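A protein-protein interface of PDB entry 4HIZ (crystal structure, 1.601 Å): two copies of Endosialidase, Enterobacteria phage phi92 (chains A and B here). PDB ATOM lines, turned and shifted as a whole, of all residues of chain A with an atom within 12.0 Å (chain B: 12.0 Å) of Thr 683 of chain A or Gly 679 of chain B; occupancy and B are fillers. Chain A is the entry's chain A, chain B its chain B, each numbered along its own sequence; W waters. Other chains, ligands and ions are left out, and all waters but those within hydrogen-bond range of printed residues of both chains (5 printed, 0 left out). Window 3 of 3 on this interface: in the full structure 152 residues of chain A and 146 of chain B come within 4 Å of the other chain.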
ATOM      1  N   PRO A 656      17.258  -3.279  -1.197  1.00  0.00           N
ATOM      2  CA  PRO A 656      17.365  -3.530  -2.632  1.00  0.00           C
ATOM      3  C   PRO A 656      15.954  -3.635  -3.227  1.00  0.00           C
ATOM      4  O   PRO A 656      15.020  -4.106  -2.564  1.00  0.00           O
ATOM      5  CB  PRO A 656      18.073  -4.893  -2.697  1.00  0.00           C
ATOM      6  CG  PRO A 656      17.609  -5.620  -1.432  1.00  0.00           C
ATOM      7  CD  PRO A 656      17.499  -4.490  -0.382  1.00  0.00           C
ATOM      8  N   LEU A 658      14.961  -5.507  -5.928  1.00  0.00           N
ATOM      9  CA  LEU A 658      14.710  -6.932  -6.157  1.00  0.00           C
ATOM     10  C   LEU A 658      15.171  -7.725  -4.944  1.00  0.00           C
ATOM     11  O   LEU A 658      16.067  -7.293  -4.221  1.00  0.00           O
ATOM     12  CB  LEU A 658      15.432  -7.415  -7.413  1.00  0.00           C
ATOM     13  CG  LEU A 658      14.909  -6.814  -8.714  1.00  0.00           C
ATOM     14  CD1 LEU A 658      15.802  -7.175  -9.867  1.00  0.00           C
ATOM     15  CD2 LEU A 658      13.496  -7.279  -8.945  1.00  0.00           C
ATOM     16  N   ASP A 659      14.517  -8.856  -4.690  1.00  0.00           N
ATOM     17  CA  ASP A 659      14.834  -9.717  -3.559  1.00  0.00           C
ATOM     18  C   ASP A 659      15.898 -10.723  -3.997  1.00  0.00           C
ATOM     19  O   ASP A 659      15.758 -11.356  -5.060  1.00  0.00           O
ATOM     20  CB  ASP A 659      13.531 -10.424  -3.158  1.00  0.00           C
ATOM     21  CG  ASP A 659      13.647 -11.278  -1.899  1.00  0.00           C
ATOM     22  OD1 ASP A 659      14.337 -10.914  -0.934  1.00  0.00           O
ATOM     23  OD2 ASP A 659      12.973 -12.344  -1.888  1.00  0.00           O
ATOM     24  N   GLY A 660      16.958 -10.839  -3.191  1.00  0.00           N
ATOM     25  CA  GLY A 660      17.995 -11.848  -3.378  1.00  0.00           C
ATOM     26  C   GLY A 660      18.884 -11.679  -4.589  1.00  0.00           C
ATOM     27  O   GLY A 660      19.488 -12.675  -5.023  1.00  0.00           O
ATOM     28  N   GLN A 661      19.016 -10.461  -5.130  1.00  0.00           N
ATOM     29  CA  GLN A 661      19.756 -10.286  -6.405  1.00  0.00           C
ATOM     30  C   GLN A 661      20.858  -9.217  -6.403  1.00  0.00           C
ATOM     31  O   GLN A 661      21.719  -9.214  -7.293  1.00  0.00           O
ATOM     32  CB  GLN A 661      18.782  -9.973  -7.532  1.00  0.00           C
ATOM     33  CG  GLN A 661      17.807 -11.115  -7.772  1.00  0.00           C
ATOM     34  CD  GLN A 661      16.826 -10.808  -8.862  1.00  0.00           C
ATOM     35  OE1 GLN A 661      17.211 -10.425  -9.973  1.00  0.00           O
ATOM     36  NE2 GLN A 661      15.540 -10.970  -8.560  1.00  0.00           N
ATOM     37  N   VAL A 662      20.838  -8.348  -5.394  1.00  0.00           N
ATOM     38  CA  VAL A 662      21.660  -7.137  -5.337  1.00  0.00           C
ATOM     39  C   VAL A 662      22.585  -7.285  -4.131  1.00  0.00           C
ATOM     40  O   VAL A 662      22.117  -7.580  -3.036  1.00  0.00           O
ATOM     41  CB  VAL A 662      20.715  -5.905  -5.038  1.00  0.00           C
ATOM     42  CG1 VAL A 662      21.494  -4.641  -4.892  1.00  0.00           C
ATOM     43  CG2 VAL A 662      19.668  -5.757  -6.127  1.00  0.00           C
ATOM     44  N   LEU A 664      25.284  -6.124  -1.097  1.00  0.00           N
ATOM     45  CA  LEU A 664      25.569  -5.002  -0.192  1.00  0.00           C
ATOM     46  C   LEU A 664      27.072  -5.053   0.047  1.00  0.00           C
ATOM     47  O   LEU A 664      27.581  -5.935   0.750  1.00  0.00           O
ATOM     48  CB  LEU A 664      24.806  -5.239   1.099  1.00  0.00           C
ATOM     49  CG  LEU A 664      24.883  -4.132   2.144  1.00  0.00           C
ATOM     50  CD1 LEU A 664      24.523  -2.787   1.482  1.00  0.00           C
ATOM     51  CD2 LEU A 664      23.901  -4.495   3.280  1.00  0.00           C
ATOM     52  N   VAL A 674      29.904  -3.554   9.953  1.00  0.00           N
ATOM     53  CA  VAL A 674      28.463  -3.358   9.866  1.00  0.00           C
ATOM     54  C   VAL A 674      27.930  -3.227  11.286  1.00  0.00           C
ATOM     55  O   VAL A 674      28.286  -4.029  12.154  1.00  0.00           O
ATOM     56  CB  VAL A 674      27.774  -4.582   9.152  1.00  0.00           C
ATOM     57  CG1 VAL A 674      26.267  -4.382   9.095  1.00  0.00           C
ATOM     58  CG2 VAL A 674      28.340  -4.767   7.746  1.00  0.00           C
ATOM     59  N   ALA A 676      24.557  -3.035  13.728  1.00  0.00           N
ATOM     60  CA  ALA A 676      23.104  -3.285  13.771  1.00  0.00           C
ATOM     61  C   ALA A 676      22.709  -3.731  15.173  1.00  0.00           C
ATOM     62  O   ALA A 676      23.538  -4.251  15.910  1.00  0.00           O
ATOM     63  CB  ALA A 676      22.669  -4.332  12.731  1.00  0.00           C
ATOM     64  N   THR A 678      20.806  -6.093  16.181  1.00  0.00           N
ATOM     65  CA  THR A 678      20.981  -7.527  16.349  1.00  0.00           C
ATOM     66  C   THR A 678      22.077  -7.979  15.421  1.00  0.00           C
ATOM     67  O   THR A 678      22.147  -7.522  14.278  1.00  0.00           O
ATOM     68  CB  THR A 678      19.696  -8.335  16.105  1.00  0.00           C
ATOM     69  OG1 THR A 678      20.033  -9.729  16.059  1.00  0.00           O
ATOM     70  CG2 THR A 678      18.987  -7.939  14.799  1.00  0.00           C
ATOM     71  N   GLY A 679      22.936  -8.866  15.924  1.00  0.00           N
ATOM     72  CA  GLY A 679      24.070  -9.346  15.162  1.00  0.00           C
ATOM     73  C   GLY A 679      23.785 -10.537  14.268  1.00  0.00           C
ATOM     74  O   GLY A 679      24.683 -11.045  13.604  1.00  0.00           O
ATOM     75  N   THR A 680      22.538 -10.994  14.247  1.00  0.00           N
ATOM     76  CA  THR A 680      22.150 -12.097  13.372  1.00  0.00           C
ATOM     77  C   THR A 680      21.450 -11.568  12.140  1.00  0.00           C
ATOM     78  O   THR A 680      20.455 -10.860  12.256  1.00  0.00           O
ATOM     79  CB  THR A 680      21.213 -13.055  14.107  1.00  0.00           C
ATOM     80  OG1 THR A 680      21.886 -13.549  15.274  1.00  0.00           O
ATOM     81  CG2 THR A 680      20.802 -14.211  13.199  1.00  0.00           C
ATOM     82  N   ILE A 681      21.982 -11.893  10.953  1.00  0.00           N
ATOM     83  CA  ILE A 681      21.321 -11.494   9.707  1.00  0.00           C
ATOM     84  C   ILE A 681      20.030 -12.292   9.554  1.00  0.00           C
ATOM     85  O   ILE A 681      20.020 -13.507   9.751  1.00  0.00           O
ATOM     86  CB  ILE A 681      22.238 -11.723   8.501  1.00  0.00           C
ATOM     87  CG1 ILE A 681      23.399 -10.727   8.541  1.00  0.00           C
ATOM     88  CG2 ILE A 681      21.481 -11.621   7.156  1.00  0.00           C
ATOM     89  CD1 ILE A 681      24.480 -11.006   7.502  1.00  0.00           C
ATOM     90  N   ASN A 682      18.947 -11.591   9.235  1.00  0.00           N
ATOM     91  CA  ASN A 682      17.658 -12.210   8.980  1.00  0.00           C
ATOM     92  C   ASN A 682      17.598 -12.694   7.537  1.00  0.00           C
ATOM     93  O   ASN A 682      17.713 -11.903   6.610  1.00  0.00           O
ATOM     94  CB  ASN A 682      16.561 -11.179   9.234  1.00  0.00           C
ATOM     95  CG  ASN A 682      15.179 -11.795   9.319  1.00  0.00           C
ATOM     96  OD1 ASN A 682      14.791 -12.595   8.469  1.00  0.00           O
ATOM     97  ND2 ASN A 682      14.422 -11.427  10.345  1.00  0.00           N
ATOM     98  N   THR A 683      17.390 -13.992   7.339  1.00  0.00           N
ATOM     99  CA  THR A 683      17.464 -14.541   5.992  1.00  0.00           C
ATOM    100  C   THR A 683      16.071 -14.654   5.390  1.00  0.00           C
ATOM    101  O   THR A 683      15.079 -14.119   5.953  1.00  0.00           O
ATOM    102  CB  THR A 683      18.153 -15.916   5.969  1.00  0.00           C
ATOM    103  OG1 THR A 683      17.467 -16.807   6.860  1.00  0.00           O
ATOM    104  CG2 THR A 683      19.639 -15.774   6.381  1.00  0.00           C
ATOM    105  OXT THR A 683      15.920 -15.271   4.329  1.00  0.00           O
ATOM    106  N   SER B 672      18.327  -1.418  12.574  1.00  0.00           N
ATOM    107  CA  SER B 672      17.588  -2.306  13.479  1.00  0.00           C
ATOM    108  C   SER B 672      17.958  -3.777  13.237  1.00  0.00           C
ATOM    109  O   SER B 672      18.140  -4.551  14.177  1.00  0.00           O
ATOM    110  CB  SER B 672      16.086  -2.112  13.305  1.00  0.00           C
ATOM    111  OG  SER B 672      15.675  -2.368  11.976  1.00  0.00           O
ATOM    112  N   GLU B 673      18.067  -4.146  11.964  1.00  0.00           N
ATOM    113  CA  GLU B 673      18.268  -5.517  11.575  1.00  0.00           C
ATOM    114  C   GLU B 673      18.682  -5.486  10.120  1.00  0.00           C
ATOM    115  O   GLU B 673      18.274  -4.595   9.366  1.00  0.00           O
ATOM    116  CB  GLU B 673      16.929  -6.284  11.718  1.00  0.00           C
ATOM    117  CG  GLU B 673      17.020  -7.809  11.520  1.00  0.00           C
ATOM    118  CD  GLU B 673      15.814  -8.547  12.113  1.00  0.00           C
ATOM    119  OE1 GLU B 673      14.817  -7.885  12.477  1.00  0.00           O
ATOM    120  OE2 GLU B 673      15.854  -9.791  12.221  1.00  0.00           O
ATOM    121  N   VAL B 674      19.513  -6.446   9.743  1.00  0.00           N
ATOM    122  CA  VAL B 674      19.991  -6.622   8.361  1.00  0.00           C
ATOM    123  C   VAL B 674      19.337  -7.862   7.756  1.00  0.00           C
ATOM    124  O   VAL B 674      19.344  -8.920   8.358  1.00  0.00           O
ATOM    125  CB  VAL B 674      21.530  -6.790   8.361  1.00  0.00           C
ATOM    126  CG1 VAL B 674      22.074  -6.879   6.948  1.00  0.00           C
ATOM    127  CG2 VAL B 674      22.179  -5.611   9.126  1.00  0.00           C
ATOM    128  N   TYR B 675      18.782  -7.721   6.560  1.00  0.00           N
ATOM    129  CA  TYR B 675      18.150  -8.842   5.856  1.00  0.00           C
ATOM    130  C   TYR B 675      18.942  -9.226   4.601  1.00  0.00           C
ATOM    131  O   TYR B 675      19.187  -8.371   3.746  1.00  0.00           O
ATOM    132  CB  TYR B 675      16.747  -8.454   5.414  1.00  0.00           C
ATOM    133  CG  TYR B 675      15.773  -8.211   6.529  1.00  0.00           C
ATOM    134  CD1 TYR B 675      15.812  -7.035   7.279  1.00  0.00           C
ATOM    135  CD2 TYR B 675      14.787  -9.155   6.811  1.00  0.00           C
ATOM    136  CE1 TYR B 675      14.886  -6.798   8.307  1.00  0.00           C
ATOM    137  CE2 TYR B 675      13.872  -8.937   7.837  1.00  0.00           C
ATOM    138  CZ  TYR B 675      13.927  -7.752   8.573  1.00  0.00           C
ATOM    139  OH  TYR B 675      13.006  -7.541   9.572  1.00  0.00           O
ATOM    140  N   ALA B 676      19.331 -10.501   4.480  1.00  0.00           N
ATOM    141  CA  ALA B 676      20.136 -10.945   3.344  1.00  0.00           C
ATOM    142  C   ALA B 676      19.851 -12.410   3.056  1.00  0.00           C
ATOM    143  O   ALA B 676      19.447 -13.155   3.955  1.00  0.00           O
ATOM    144  CB  ALA B 676      21.643 -10.719   3.616  1.00  0.00           C
ATOM    145  N   SER B 677      20.065 -12.841   1.815  1.00  0.00           N
ATOM    146  CA  SER B 677      19.700 -14.223   1.463  1.00  0.00           C
ATOM    147  C   SER B 677      20.597 -15.224   2.181  1.00  0.00           C
ATOM    148  O   SER B 677      20.157 -16.339   2.482  1.00  0.00           O
ATOM    149  CB  SER B 677      19.791 -14.434  -0.043  1.00  0.00           C
ATOM    150  OG  SER B 677      18.925 -13.545  -0.725  1.00  0.00           O
ATOM    151  N   THR B 678      21.855 -14.834   2.426  1.00  0.00           N
ATOM    152  CA  THR B 678      22.754 -15.639   3.257  1.00  0.00           C
ATOM    153  C   THR B 678      23.078 -14.858   4.517  1.00  0.00           C
ATOM    154  O   THR B 678      23.293 -13.647   4.459  1.00  0.00           O
ATOM    155  CB  THR B 678      24.059 -16.112   2.530  1.00  0.00           C
ATOM    156  OG1 THR B 678      24.993 -16.615   3.502  1.00  0.00           O
ATOM    157  CG2 THR B 678      24.733 -14.979   1.770  1.00  0.00           C
ATOM    158  N   GLY B 679      23.089 -15.556   5.648  1.00  0.00           N
ATOM    159  CA  GLY B 679      23.351 -14.932   6.938  1.00  0.00           C
ATOM    160  C   GLY B 679      24.824 -14.831   7.302  1.00  0.00           C
ATOM    161  O   GLY B 679      25.158 -14.356   8.382  1.00  0.00           O
ATOM    162  N   THR B 680      25.713 -15.270   6.414  1.00  0.00           N
ATOM    163  CA  THR B 680      27.133 -15.145   6.670  1.00  0.00           C
ATOM    164  C   THR B 680      27.716 -13.988   5.872  1.00  0.00           C
ATOM    165  O   THR B 680      27.553 -13.920   4.650  1.00  0.00           O
ATOM    166  CB  THR B 680      27.882 -16.437   6.278  1.00  0.00           C
ATOM    167  OG1 THR B 680      27.371 -17.528   7.042  1.00  0.00           O
ATOM    168  CG2 THR B 680      29.409 -16.307   6.494  1.00  0.00           C
ATOM    169  N   ILE B 681      28.390 -13.069   6.562  1.00  0.00           N
ATOM    170  CA  ILE B 681      29.044 -11.962   5.870  1.00  0.00           C
ATOM    171  C   ILE B 681      30.238 -12.510   5.111  1.00  0.00           C
ATOM    172  O   ILE B 681      30.960 -13.356   5.635  1.00  0.00           O
ATOM    173  CB  ILE B 681      29.484 -10.871   6.870  1.00  0.00           C
ATOM    174  CG1 ILE B 681      28.239 -10.157   7.408  1.00  0.00           C
ATOM    175  CG2 ILE B 681      30.456  -9.888   6.218  1.00  0.00           C
ATOM    176  CD1 ILE B 681      28.513  -9.153   8.582  1.00  0.00           C
ATOM    177  N   ASN B 682      30.422 -12.054   3.870  1.00  0.00           N
ATOM    178  CA  ASN B 682      31.554 -12.455   3.041  1.00  0.00           C
ATOM    179  C   ASN B 682      32.701 -11.478   3.300  1.00  0.00           C
ATOM    180  O   ASN B 682      32.540 -10.266   3.095  1.00  0.00           O
ATOM    181  CB  ASN B 682      31.115 -12.406   1.574  1.00  0.00           C
ATOM    182  CG  ASN B 682      32.134 -13.015   0.629  1.00  0.00           C
ATOM    183  OD1 ASN B 682      33.326 -12.749   0.722  1.00  0.00           O
ATOM    184  ND2 ASN B 682      31.663 -13.834  -0.285  1.00  0.00           N
ATOM    185  N   THR B 683      33.852 -11.988   3.758  1.00  0.00           N
ATOM    186  CA  THR B 683      34.934 -11.112   4.184  1.00  0.00           C
ATOM    187  C   THR B 683      35.955 -10.895   3.063  1.00  0.00           C
ATOM    188  O   THR B 683      35.715 -11.306   1.910  1.00  0.00           O
ATOM    189  CB  THR B 683      35.657 -11.659   5.438  1.00  0.00           C
ATOM    190  OG1 THR B 683      36.134 -12.986   5.166  1.00  0.00           O
ATOM    191  CG2 THR B 683      34.712 -11.715   6.615  1.00  0.00           C
ATOM    192  OXT THR B 683      37.025 -10.304   3.290  1.00  0.00           O
HETATM  193  O   HOH W   1      17.827 -11.542  12.766  1.00  0.00           O
HETATM  194  O   HOH W   2      20.922  -8.050  11.760  1.00  0.00           O
HETATM  195  O   HOH W   3      17.387 -16.851   2.457  1.00  0.00           O
HETATM  196  O   HOH W   4      24.065 -13.672  10.772  1.00  0.00           O
HETATM  197  O   HOH W   5      19.875 -15.069  -3.622  1.00  0.00           O
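The backbone NH of Thr 680 of chain A lies close to the side-chain hydroxyl of Thr 678 of chain A (3.3 Å). The side-chain carboxylate of Glu 673 of chain B sits at hydrogen-bond distance from the side-chain hydroxyl of Tyr 675 of chain B, 3.4 Å away. The backbone NH of Thr 680 of chain B sits close to the side-chain hydroxyl of Thr 678 of chain B (3.3 Å).
Of the 12 printed residues of chain B, 9 touch a printed residue of chain A. Of the 15 printed residues of chain A, 6 touch a printed residue of chain B. Printed residues of chain A that touch a printed residue of chain B: Gly 660, Ala 676, Thr 678, Ile 681, Asn 682 and Thr 683. Hydrophobic or aromatic side chains of chain A that line the printed part of chain B: Ala 676 and Ile 681. Along chain A the printed residues that touch a printed residue of chain B span positions 660 to 683.
Of the printed residues of chain B, Thr 683 of chain A touches Ala 676 (3.2 Å), Ser 677 (3.97 Å) and Gly 679 (3.5 Å). Of chain B, only Glu 673 (2.9 Å), Val 674 (2.8 Å), Tyr 675 (3.2 Å) and Ala 676 (3.0 Å) come within 4 Å of Asn 682 of chain A. Printed residues of chain A within 4 Å of Tyr 675 of chain B: Asn 682. Of chain A, only Ile 681, Asn 682 and Thr 683 come within 4 Å of Ala 676 of chain B. Ser 677 of chain B touches just these residues of chain A: Gly 660 and Thr 683. No residue of chain A comes within 4 Å of Thr 680 of chain B. Of the printed residues of chain A, Thr 678 of chain B touches Ile 681 (3.8 Å). Printed residues of chain A within 4 Å of Glu 673 of chain B: Thr 678 and Asn 682. The nearest printed residue of chain A that does not touch Gly 679 of chain B is Thr 680 of chain A (6.0 Å).
The side-chain amide nitrogen (ND2) of Asn 682 of chain A sits at hydrogen-bond distance from the side-chain carboxylate (OE2) of Glu 673 of chain B (2.9 Å). The backbone carbonyl oxygen of Val 674 of chain B lies within hydrogen-bond range of the backbone NH of Asn 682 of chain A, at 2.8 Å. The backbone NH of Ala 676 of chain B lies within hydrogen-bond range of the backbone carbonyl oxygen of Asn 682 of chain A, at 3.0 Å.
Ile 681 of chain A touches Val 674 of chain B, but with the chains exchanged Val 674 of chain A does not touch Ile 681 of chain B (4.5 Å). Ile 681 of chain A touches Thr 678 of chain B, but with the chains exchanged Thr 678 of chain A does not touch Ile 681 of chain B (8.7 Å). Ile 681 of chain A touches its own counterpart, Ile 681 of chain B. Thr 683 of chain A touches Gly 679 of chain B, but with the chains exchanged Gly 679 of chain A does not touch Thr 683 of chain B (12.2 Å). 8 positions are printed for both chains. Of the 16 pairs that touch across the chains among the printed residues, 1 has its exchanged pair printed and touching as well.
Ser 677 of chain B touches Gly 660 of chain A. Ser 672 of chain B touches Thr 678 of chain A (O to CG2, 3.5 Å). CG of Glu 673 of chain B touches CG2 of Thr 678 of chain A, 3.8 Å away. Ile 681 of chain A touches Val 674 of chain B (CA to O, 3.5 Å). Ile 681 of chain A touches Ala 676 of chain B. O of Thr 678 of chain B touches CG2 of Ile 681 of chain A, at 3.8 Å. CG1 of Ile 681 of chain B touches CD1 of Ile 681 of chain A (3.9 Å). Asn 682 of chain A touches Tyr 675 of chain B. Thr 683 of chain A touches Ala 676 of chain B. Thr 683 of chain A touches Ser 677 of chain B (CG2 to O, 3.97 Å).
Water W1 bridges the side-chain carboxylate of Glu 673 of chain B (2.7 Å) and the backbone carbonyl oxygen of Thr 680 of chain A (2.8 Å). Water W4 lies within hydrogen-bond range of the backbone carbonyl oxygen of Gly 679 of chain B and the backbone NH of Ile 681 of chain A. Water W5 lies within hydrogen-bond range of the backbone carbonyl oxygen of Gly 660 of chain A (2.8 Å) and the side-chain hydroxyl of Ser 677 of chain B (3.4 Å). Water W3 bridges the backbone carbonyl oxygen (O) of Ser 677 of chain B (2.8 Å) and the chain-end carboxylate (OXT) of Thr 683 of chain A (2.9 Å). Water W2 lies within hydrogen-bond range of O of Thr 678 of chain A, O of Thr 680 of chain A and N of Val 674 of chain B.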
